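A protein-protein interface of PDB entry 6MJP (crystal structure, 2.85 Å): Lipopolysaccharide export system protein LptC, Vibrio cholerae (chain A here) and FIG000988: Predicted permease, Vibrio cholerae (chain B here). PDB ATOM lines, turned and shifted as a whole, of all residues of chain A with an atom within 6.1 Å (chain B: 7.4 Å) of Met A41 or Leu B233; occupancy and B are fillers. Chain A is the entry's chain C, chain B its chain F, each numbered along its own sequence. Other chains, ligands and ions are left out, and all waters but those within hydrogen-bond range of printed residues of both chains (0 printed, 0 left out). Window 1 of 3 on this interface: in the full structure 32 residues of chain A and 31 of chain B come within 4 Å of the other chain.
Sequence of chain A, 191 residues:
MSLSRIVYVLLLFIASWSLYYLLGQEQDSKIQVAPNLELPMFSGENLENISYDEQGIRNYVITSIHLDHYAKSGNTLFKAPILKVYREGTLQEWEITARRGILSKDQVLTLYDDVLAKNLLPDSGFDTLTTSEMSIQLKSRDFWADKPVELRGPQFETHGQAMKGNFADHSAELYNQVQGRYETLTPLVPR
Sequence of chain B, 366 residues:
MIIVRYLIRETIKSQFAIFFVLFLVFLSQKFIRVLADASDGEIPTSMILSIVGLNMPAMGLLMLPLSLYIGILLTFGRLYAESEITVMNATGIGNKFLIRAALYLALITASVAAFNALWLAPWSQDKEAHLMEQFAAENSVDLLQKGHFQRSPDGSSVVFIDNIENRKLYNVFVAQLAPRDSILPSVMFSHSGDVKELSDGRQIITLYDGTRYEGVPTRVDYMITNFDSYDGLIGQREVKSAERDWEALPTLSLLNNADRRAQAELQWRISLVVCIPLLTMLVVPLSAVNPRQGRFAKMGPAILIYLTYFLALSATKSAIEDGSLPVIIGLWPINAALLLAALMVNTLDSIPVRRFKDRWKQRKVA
The backbone carbonyl oxygen of Ser A43 is in hydrogen-bond range of the backbone NH of Asp B231, at 2.5 Å.
The backbone carbonyl oxygen of Phe A42 lies within hydrogen-bond range of the backbone NH of His A69. The backbone NH of Met A41 lies within hydrogen-bond range of the backbone carbonyl oxygen of His A69. OD1 of Asp B231 sits close to OG1 of Thr B206 (3.4 Å).
Met A41 touches Leu B233 (O to N, 3.7 Å). CD1 of Ile B183 touches CE2 of Phe A42, at 3.6 Å. Phe A42 touches Arg B212. Phe A42 touches Asp B231 (CD1 to O, 3.7 Å). Ile B183 touches His A69. CG2 of Ile B183 touches O of Tyr A70, at 3.8 Å. CB of Asp B181 touches O of Ala A71 (3.2 Å).
Leu A39 touches none of the printed residues of chain B. Met A41 touches one residue of chain B. Of the printed residues of chain B, Tyr A70 touches Ile B183 (3.8 Å). Of the printed residues of chain A, Asp B181 touches Ala A71. Thr B206 touches none of the printed residues of chain A. Of chain A, only Met A41 (3.7 Å) comes within 4 Å of Leu B233. The nearest residue of chain A that does not touch Leu B233 is Asn A36 (4.1 Å). The nearest printed residue of chain A that does not touch Arg B212 is His A69 (5.3 Å).
Printed residues of chain B that touch a printed residue of chain A: Asp B181, Ile B183, Arg B212, Asp B231 and Leu B233. Hydrophobic or aromatic side chains of chain B that line the printed part of chain A: Ile B183. Hydrophobic or aromatic side chains of chain A that line the printed part of chain B: Phe A42 and His A69. Among the printed residues, 8 pairs touch across the chains. Among the printed residues, no Asp or Glu carboxylate lies within 4 Å of a Lys or Arg side-chain nitrogen of the other chain.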
ATOM      1  N   ASN A  36       8.092   8.662  10.048  1.00  0.00           N
ATOM      2  CA  ASN A  36       8.739   9.873  10.531  1.00  0.00           C
ATOM      3  C   ASN A  36      10.223   9.618  10.804  1.00  0.00           C
ATOM      4  O   ASN A  36      10.723   8.495  10.700  1.00  0.00           O
ATOM      5  CB  ASN A  36       8.030  10.388  11.782  1.00  0.00           C
ATOM      6  N   LEU A  39      13.194  11.847  15.938  1.00  0.00           N
ATOM      7  CA  LEU A  39      12.963  13.109  16.630  1.00  0.00           C
ATOM      8  C   LEU A  39      12.162  12.836  17.898  1.00  0.00           C
ATOM      9  O   LEU A  39      11.651  11.722  18.071  1.00  0.00           O
ATOM     10  CB  LEU A  39      12.229  14.093  15.713  1.00  0.00           C
ATOM     11  CG  LEU A  39      13.015  14.650  14.524  1.00  0.00           C
ATOM     12  CD1 LEU A  39      12.148  15.572  13.677  1.00  0.00           C
ATOM     13  CD2 LEU A  39      14.265  15.372  15.005  1.00  0.00           C
ATOM     14  N   PRO A  40      12.039  13.799  18.813  1.00  0.00           N
ATOM     15  CA  PRO A  40      11.214  13.570  20.011  1.00  0.00           C
ATOM     16  C   PRO A  40       9.768  13.285  19.642  1.00  0.00           C
ATOM     17  O   PRO A  40       9.079  14.121  19.053  1.00  0.00           O
ATOM     18  CB  PRO A  40      11.357  14.881  20.798  1.00  0.00           C
ATOM     19  CG  PRO A  40      11.891  15.879  19.814  1.00  0.00           C
ATOM     20  CD  PRO A  40      12.747  15.088  18.883  1.00  0.00           C
ATOM     21  N   MET A  41       9.309  12.085  19.997  1.00  0.00           N
ATOM     22  CA  MET A  41       7.957  11.666  19.648  1.00  0.00           C
ATOM     23  C   MET A  41       6.902  12.301  20.548  1.00  0.00           C
ATOM     24  O   MET A  41       5.758  12.483  20.120  1.00  0.00           O
ATOM     25  CB  MET A  41       7.856  10.143  19.712  1.00  0.00           C
ATOM     26  CG  MET A  41       6.619   9.573  19.052  1.00  0.00           C
ATOM     27  SD  MET A  41       6.527   7.776  19.165  1.00  0.00           S
ATOM     28  CE  MET A  41       5.123   7.455  18.100  1.00  0.00           C
ATOM     29  N   PHE A  42       7.256  12.634  21.786  1.00  0.00           N
ATOM     30  CA  PHE A  42       6.353  13.294  22.715  1.00  0.00           C
ATOM     31  C   PHE A  42       7.072  14.479  23.337  1.00  0.00           C
ATOM     32  O   PHE A  42       8.267  14.404  23.639  1.00  0.00           O
ATOM     33  CB  PHE A  42       5.866  12.338  23.820  1.00  0.00           C
ATOM     34  CG  PHE A  42       4.941  11.257  23.330  1.00  0.00           C
ATOM     35  CD1 PHE A  42       3.566  11.401  23.431  1.00  0.00           C
ATOM     36  CD2 PHE A  42       5.446  10.097  22.770  1.00  0.00           C
ATOM     37  CE1 PHE A  42       2.714  10.405  22.981  1.00  0.00           C
ATOM     38  CE2 PHE A  42       4.602   9.100  22.318  1.00  0.00           C
ATOM     39  CZ  PHE A  42       3.235   9.252  22.425  1.00  0.00           C
ATOM     40  N   SER A  43       6.341  15.572  23.516  1.00  0.00           N
ATOM     41  CA  SER A  43       6.887  16.781  24.108  1.00  0.00           C
ATOM     42  C   SER A  43       5.839  17.406  25.015  1.00  0.00           C
ATOM     43  O   SER A  43       4.639  17.293  24.766  1.00  0.00           O
ATOM     44  CB  SER A  43       7.324  17.788  23.038  1.00  0.00           C
ATOM     45  OG  SER A  43       7.846  18.961  23.637  1.00  0.00           O
ATOM     46  N   HIS A  69       9.885  12.638  25.306  1.00  0.00           N
ATOM     47  CA  HIS A  69       9.940  11.180  25.323  1.00  0.00           C
ATOM     48  C   HIS A  69      10.307  10.672  23.946  1.00  0.00           C
ATOM     49  O   HIS A  69       9.702  11.079  22.954  1.00  0.00           O
ATOM     50  CB  HIS A  69       8.597  10.584  25.750  1.00  0.00           C
ATOM     51  CG  HIS A  69       8.698   9.222  26.365  1.00  0.00           C
ATOM     52  ND1 HIS A  69       7.672   8.662  27.098  1.00  0.00           N
ATOM     53  CD2 HIS A  69       9.700   8.311  26.368  1.00  0.00           C
ATOM     54  CE1 HIS A  69       8.038   7.467  27.518  1.00  0.00           C
ATOM     55  NE2 HIS A  69       9.263   7.229  27.091  1.00  0.00           N
ATOM     56  N   TYR A  70      11.307   9.798  23.880  1.00  0.00           N
ATOM     57  CA  TYR A  70      11.740   9.231  22.610  1.00  0.00           C
ATOM     58  C   TYR A  70      11.327   7.767  22.505  1.00  0.00           C
ATOM     59  O   TYR A  70      11.208   7.064  23.514  1.00  0.00           O
ATOM     60  CB  TYR A  70      13.242   9.372  22.446  1.00  0.00           C
ATOM     61  CG  TYR A  70      13.730  10.796  22.324  1.00  0.00           C
ATOM     62  CD1 TYR A  70      13.924  11.376  21.079  1.00  0.00           C
ATOM     63  CD2 TYR A  70      14.001  11.564  23.453  1.00  0.00           C
ATOM     64  CE1 TYR A  70      14.379  12.669  20.955  1.00  0.00           C
ATOM     65  CE2 TYR A  70      14.456  12.869  23.338  1.00  0.00           C
ATOM     66  CZ  TYR A  70      14.639  13.413  22.082  1.00  0.00           C
ATOM     67  OH  TYR A  70      15.090  14.705  21.947  1.00  0.00           O
ATOM     68  N   ALA A  71      11.121   7.304  21.275  1.00  0.00           N
ATOM     69  CA  ALA A  71      10.608   5.960  21.032  1.00  0.00           C
ATOM     70  C   ALA A  71      11.693   4.913  20.797  1.00  0.00           C
ATOM     71  O   ALA A  71      11.619   3.826  21.377  1.00  0.00           O
ATOM     72  CB  ALA A  71       9.655   5.969  19.831  1.00  0.00           C
ATOM     73  N   SER B 152      -5.621   7.691  14.106  1.00  0.00           N
ATOM     74  CA  SER B 152      -4.657   8.535  13.421  1.00  0.00           C
ATOM     75  C   SER B 152      -4.036   7.801  12.240  1.00  0.00           C
ATOM     76  O   SER B 152      -4.047   6.570  12.195  1.00  0.00           O
ATOM     77  CB  SER B 152      -3.564   8.968  14.385  1.00  0.00           C
ATOM     78  OG  SER B 152      -4.114   9.712  15.454  1.00  0.00           O
ATOM     79  N   ASP B 154      -1.160   7.099  11.850  1.00  0.00           N
ATOM     80  CA  ASP B 154      -0.281   6.092  12.429  1.00  0.00           C
ATOM     81  C   ASP B 154      -1.047   4.809  12.725  1.00  0.00           C
ATOM     82  O   ASP B 154      -0.516   3.709  12.541  1.00  0.00           O
ATOM     83  CB  ASP B 154       0.382   6.634  13.700  1.00  0.00           C
ATOM     84  CG  ASP B 154       1.433   7.690  13.406  1.00  0.00           C
ATOM     85  OD1 ASP B 154       1.642   8.000  12.216  1.00  0.00           O
ATOM     86  OD2 ASP B 154       2.047   8.214  14.362  1.00  0.00           O
ATOM     87  N   SER B 156      -1.792   3.819  15.661  1.00  0.00           N
ATOM     88  CA  SER B 156      -1.415   3.368  16.993  1.00  0.00           C
ATOM     89  C   SER B 156      -2.156   4.089  18.112  1.00  0.00           C
ATOM     90  O   SER B 156      -2.058   3.662  19.269  1.00  0.00           O
ATOM     91  CB  SER B 156       0.089   3.548  17.197  1.00  0.00           C
ATOM     92  OG  SER B 156       0.453   4.897  16.974  1.00  0.00           O
ATOM     93  N   SER B 157      -2.872   5.171  17.807  1.00  0.00           N
ATOM     94  CA  SER B 157      -3.642   5.906  18.799  1.00  0.00           C
ATOM     95  C   SER B 157      -5.083   6.043  18.332  1.00  0.00           C
ATOM     96  O   SER B 157      -5.345   6.243  17.142  1.00  0.00           O
ATOM     97  CB  SER B 157      -3.040   7.298  19.071  1.00  0.00           C
ATOM     98  OG  SER B 157      -2.966   8.084  17.896  1.00  0.00           O
ATOM     99  N   GLN B 176      -4.130   4.590  23.639  1.00  0.00           N
ATOM    100  CA  GLN B 176      -3.055   3.889  22.937  1.00  0.00           C
ATOM    101  C   GLN B 176      -2.819   2.574  23.671  1.00  0.00           C
ATOM    102  O   GLN B 176      -2.123   2.537  24.689  1.00  0.00           O
ATOM    103  CB  GLN B 176      -1.788   4.733  22.869  1.00  0.00           C
ATOM    104  CG  GLN B 176      -0.582   4.004  22.309  1.00  0.00           C
ATOM    105  CD  GLN B 176       0.689   4.827  22.390  1.00  0.00           C
ATOM    106  OE1 GLN B 176       0.648   6.057  22.334  1.00  0.00           O
ATOM    107  NE2 GLN B 176       1.825   4.151  22.530  1.00  0.00           N
ATOM    108  N   ARG B 180       4.498   1.208  21.228  1.00  0.00           N
ATOM    109  CA  ARG B 180       5.464   1.528  20.190  1.00  0.00           C
ATOM    110  C   ARG B 180       6.809   0.985  20.674  1.00  0.00           C
ATOM    111  O   ARG B 180       6.871   0.202  21.626  1.00  0.00           O
ATOM    112  CB  ARG B 180       5.440   3.028  19.887  1.00  0.00           C
ATOM    113  N   ASP B 181       7.897   1.381  20.008  1.00  0.00           N
ATOM    114  CA  ASP B 181       9.194   0.726  20.190  1.00  0.00           C
ATOM    115  C   ASP B 181       9.526   0.485  21.659  1.00  0.00           C
ATOM    116  O   ASP B 181       9.653  -0.661  22.103  1.00  0.00           O
ATOM    117  CB  ASP B 181      10.298   1.555  19.531  1.00  0.00           C
ATOM    118  N   ILE B 183       8.032   2.780  24.219  1.00  0.00           N
ATOM    119  CA  ILE B 183       7.057   3.499  25.033  1.00  0.00           C
ATOM    120  C   ILE B 183       5.918   2.559  25.404  1.00  0.00           C
ATOM    121  O   ILE B 183       5.470   1.736  24.595  1.00  0.00           O
ATOM    122  CB  ILE B 183       6.528   4.750  24.308  1.00  0.00           C
ATOM    123  CG1 ILE B 183       5.732   4.350  23.074  1.00  0.00           C
ATOM    124  CG2 ILE B 183       7.670   5.692  23.934  1.00  0.00           C
ATOM    125  CD1 ILE B 183       5.156   5.514  22.336  1.00  0.00           C
ATOM    126  N   GLY B 201       6.763  18.114   7.522  1.00  0.00           N
ATOM    127  CA  GLY B 201       6.550  16.790   6.976  1.00  0.00           C
ATOM    128  C   GLY B 201       5.759  15.826   7.834  1.00  0.00           C
ATOM    129  O   GLY B 201       5.652  14.651   7.469  1.00  0.00           O
ATOM    130  N   ARG B 202       5.186  16.278   8.955  1.00  0.00           N
ATOM    131  CA  ARG B 202       4.484  15.405   9.891  1.00  0.00           C
ATOM    132  C   ARG B 202       3.196  16.077  10.360  1.00  0.00           C
ATOM    133  O   ARG B 202       2.957  17.261  10.106  1.00  0.00           O
ATOM    134  CB  ARG B 202       5.364  15.051  11.095  1.00  0.00           C
ATOM    135  N   GLN B 203       2.360  15.304  11.050  1.00  0.00           N
ATOM    136  CA  GLN B 203       1.093  15.778  11.596  1.00  0.00           C
ATOM    137  C   GLN B 203       1.133  15.588  13.103  1.00  0.00           C
ATOM    138  O   GLN B 203       1.407  14.482  13.578  1.00  0.00           O
ATOM    139  CB  GLN B 203      -0.095  15.015  10.992  1.00  0.00           C
ATOM    140  CG  GLN B 203       0.118  14.580   9.545  1.00  0.00           C
ATOM    141  CD  GLN B 203      -0.871  13.514   9.099  1.00  0.00           C
ATOM    142  OE1 GLN B 203      -0.479  12.415   8.702  1.00  0.00           O
ATOM    143  NE2 GLN B 203      -2.160  13.835   9.158  1.00  0.00           N
ATOM    144  N   ILE B 204       0.883  16.660  13.857  1.00  0.00           N
ATOM    145  CA  ILE B 204       1.008  16.619  15.308  1.00  0.00           C
ATOM    146  C   ILE B 204      -0.295  17.081  15.949  1.00  0.00           C
ATOM    147  O   ILE B 204      -1.151  17.701  15.315  1.00  0.00           O
ATOM    148  CB  ILE B 204       2.188  17.476  15.821  1.00  0.00           C
ATOM    149  CG1 ILE B 204       2.143  18.868  15.193  1.00  0.00           C
ATOM    150  CG2 ILE B 204       3.520  16.798  15.534  1.00  0.00           C
ATOM    151  CD1 ILE B 204       3.316  19.734  15.583  1.00  0.00           C
ATOM    152  N   ILE B 205      -0.428  16.764  17.235  1.00  0.00           N
ATOM    153  CA  ILE B 205      -1.568  17.155  18.057  1.00  0.00           C
ATOM    154  C   ILE B 205      -1.031  17.625  19.400  1.00  0.00           C
ATOM    155  O   ILE B 205      -0.065  17.063  19.921  1.00  0.00           O
ATOM    156  CB  ILE B 205      -2.568  15.989  18.238  1.00  0.00           C
ATOM    157  CG1 ILE B 205      -3.717  16.367  19.171  1.00  0.00           C
ATOM    158  CG2 ILE B 205      -1.880  14.769  18.811  1.00  0.00           C
ATOM    159  CD1 ILE B 205      -4.789  15.290  19.277  1.00  0.00           C
ATOM    160  N   THR B 206      -1.634  18.670  19.953  1.00  0.00           N
ATOM    161  CA  THR B 206      -1.276  19.147  21.280  1.00  0.00           C
ATOM    162  C   THR B 206      -2.493  19.043  22.195  1.00  0.00           C
ATOM    163  O   THR B 206      -3.623  19.200  21.735  1.00  0.00           O
ATOM    164  CB  THR B 206      -0.758  20.591  21.221  1.00  0.00           C
ATOM    165  OG1 THR B 206      -0.488  21.063  22.546  1.00  0.00           O
ATOM    166  CG2 THR B 206      -1.771  21.504  20.548  1.00  0.00           C
ATOM    167  N   ARG B 212      -2.201  12.360  31.797  1.00  0.00           N
ATOM    168  CA  ARG B 212      -1.898  11.164  31.022  1.00  0.00           C
ATOM    169  C   ARG B 212      -1.622  10.003  31.967  1.00  0.00           C
ATOM    170  O   ARG B 212      -0.933  10.176  32.974  1.00  0.00           O
ATOM    171  CB  ARG B 212      -0.691  11.385  30.111  1.00  0.00           C
ATOM    172  CG  ARG B 212      -0.076  10.102  29.612  1.00  0.00           C
ATOM    173  CD  ARG B 212       0.864  10.345  28.462  1.00  0.00           C
ATOM    174  NE  ARG B 212       1.354   9.087  27.917  1.00  0.00           N
ATOM    175  CZ  ARG B 212       2.053   8.979  26.794  1.00  0.00           C
ATOM    176  NH1 ARG B 212       2.343  10.061  26.086  1.00  0.00           N
ATOM    177  NH2 ARG B 212       2.460   7.790  26.380  1.00  0.00           N
ATOM    178  N   ASP B 231       2.378  17.503  23.669  1.00  0.00           N
ATOM    179  CA  ASP B 231       2.328  17.234  22.238  1.00  0.00           C
ATOM    180  C   ASP B 231       2.357  15.735  21.964  1.00  0.00           C
ATOM    181  O   ASP B 231       2.736  14.926  22.814  1.00  0.00           O
ATOM    182  CB  ASP B 231       3.500  17.907  21.519  1.00  0.00           C
ATOM    183  CG  ASP B 231       3.433  19.416  21.577  1.00  0.00           C
ATOM    184  OD1 ASP B 231       2.397  19.980  21.168  1.00  0.00           O
ATOM    185  OD2 ASP B 231       4.411  20.038  22.040  1.00  0.00           O
ATOM    186  N   GLY B 232       1.964  15.378  20.745  1.00  0.00           N
ATOM    187  CA  GLY B 232       1.960  13.990  20.321  1.00  0.00           C
ATOM    188  C   GLY B 232       1.957  13.896  18.816  1.00  0.00           C
ATOM    189  O   GLY B 232       1.481  14.801  18.124  1.00  0.00           O
ATOM    190  N   LEU B 233       2.499  12.794  18.301  1.00  0.00           N
ATOM    191  CA  LEU B 233       2.604  12.592  16.862  1.00  0.00           C
ATOM    192  C   LEU B 233       1.370  11.871  16.337  1.00  0.00           C
ATOM    193  O   LEU B 233       0.902  10.901  16.935  1.00  0.00           O
ATOM    194  CB  LEU B 233       3.860  11.792  16.510  1.00  0.00           C
ATOM    195  CG  LEU B 233       4.078  11.525  15.014  1.00  0.00           C
ATOM    196  CD1 LEU B 233       4.270  12.824  14.245  1.00  0.00           C
ATOM    197  CD2 LEU B 233       5.251  10.589  14.772  1.00  0.00           C
ATOM    198  N   ILE B 234       0.848  12.351  15.211  1.00  0.00           N
ATOM    199  CA  ILE B 234      -0.328  11.772  14.586  1.00  0.00           C
ATOM    200  C   ILE B 234       0.023  11.039  13.296  1.00  0.00           C
ATOM    201  O   ILE B 234      -0.446   9.922  13.070  1.00  0.00           O
ATOM    202  CB  ILE B 234      -1.396  12.861  14.337  1.00  0.00           C
ATOM    203  CG1 ILE B 234      -2.216  13.104  15.604  1.00  0.00           C
ATOM    204  CG2 ILE B 234      -2.307  12.506  13.157  1.00  0.00           C
ATOM    205  CD1 ILE B 234      -3.451  13.936  15.363  1.00  0.00           C
ATOM    206  N   GLY B 235       0.851  11.636  12.449  1.00  0.00           N
ATOM    207  CA  GLY B 235       1.190  11.003  11.189  1.00  0.00           C
ATOM    208  C   GLY B 235       2.223  11.817  10.448  1.00  0.00           C
ATOM    209  O   GLY B 235       2.648  12.888  10.896  1.00  0.00           O
ATOM    210  N   GLN B 236       2.622  11.287   9.295  1.00  0.00           N
ATOM    211  CA  GLN B 236       3.603  11.941   8.436  1.00  0.00           C
ATOM    212  C   GLN B 236       3.497  11.432   6.996  1.00  0.00           C
ATOM    213  O   GLN B 236       3.167  12.183   6.077  1.00  0.00           O
ATOM    214  CB  GLN B 236       5.020  11.716   8.976  1.00  0.00           C
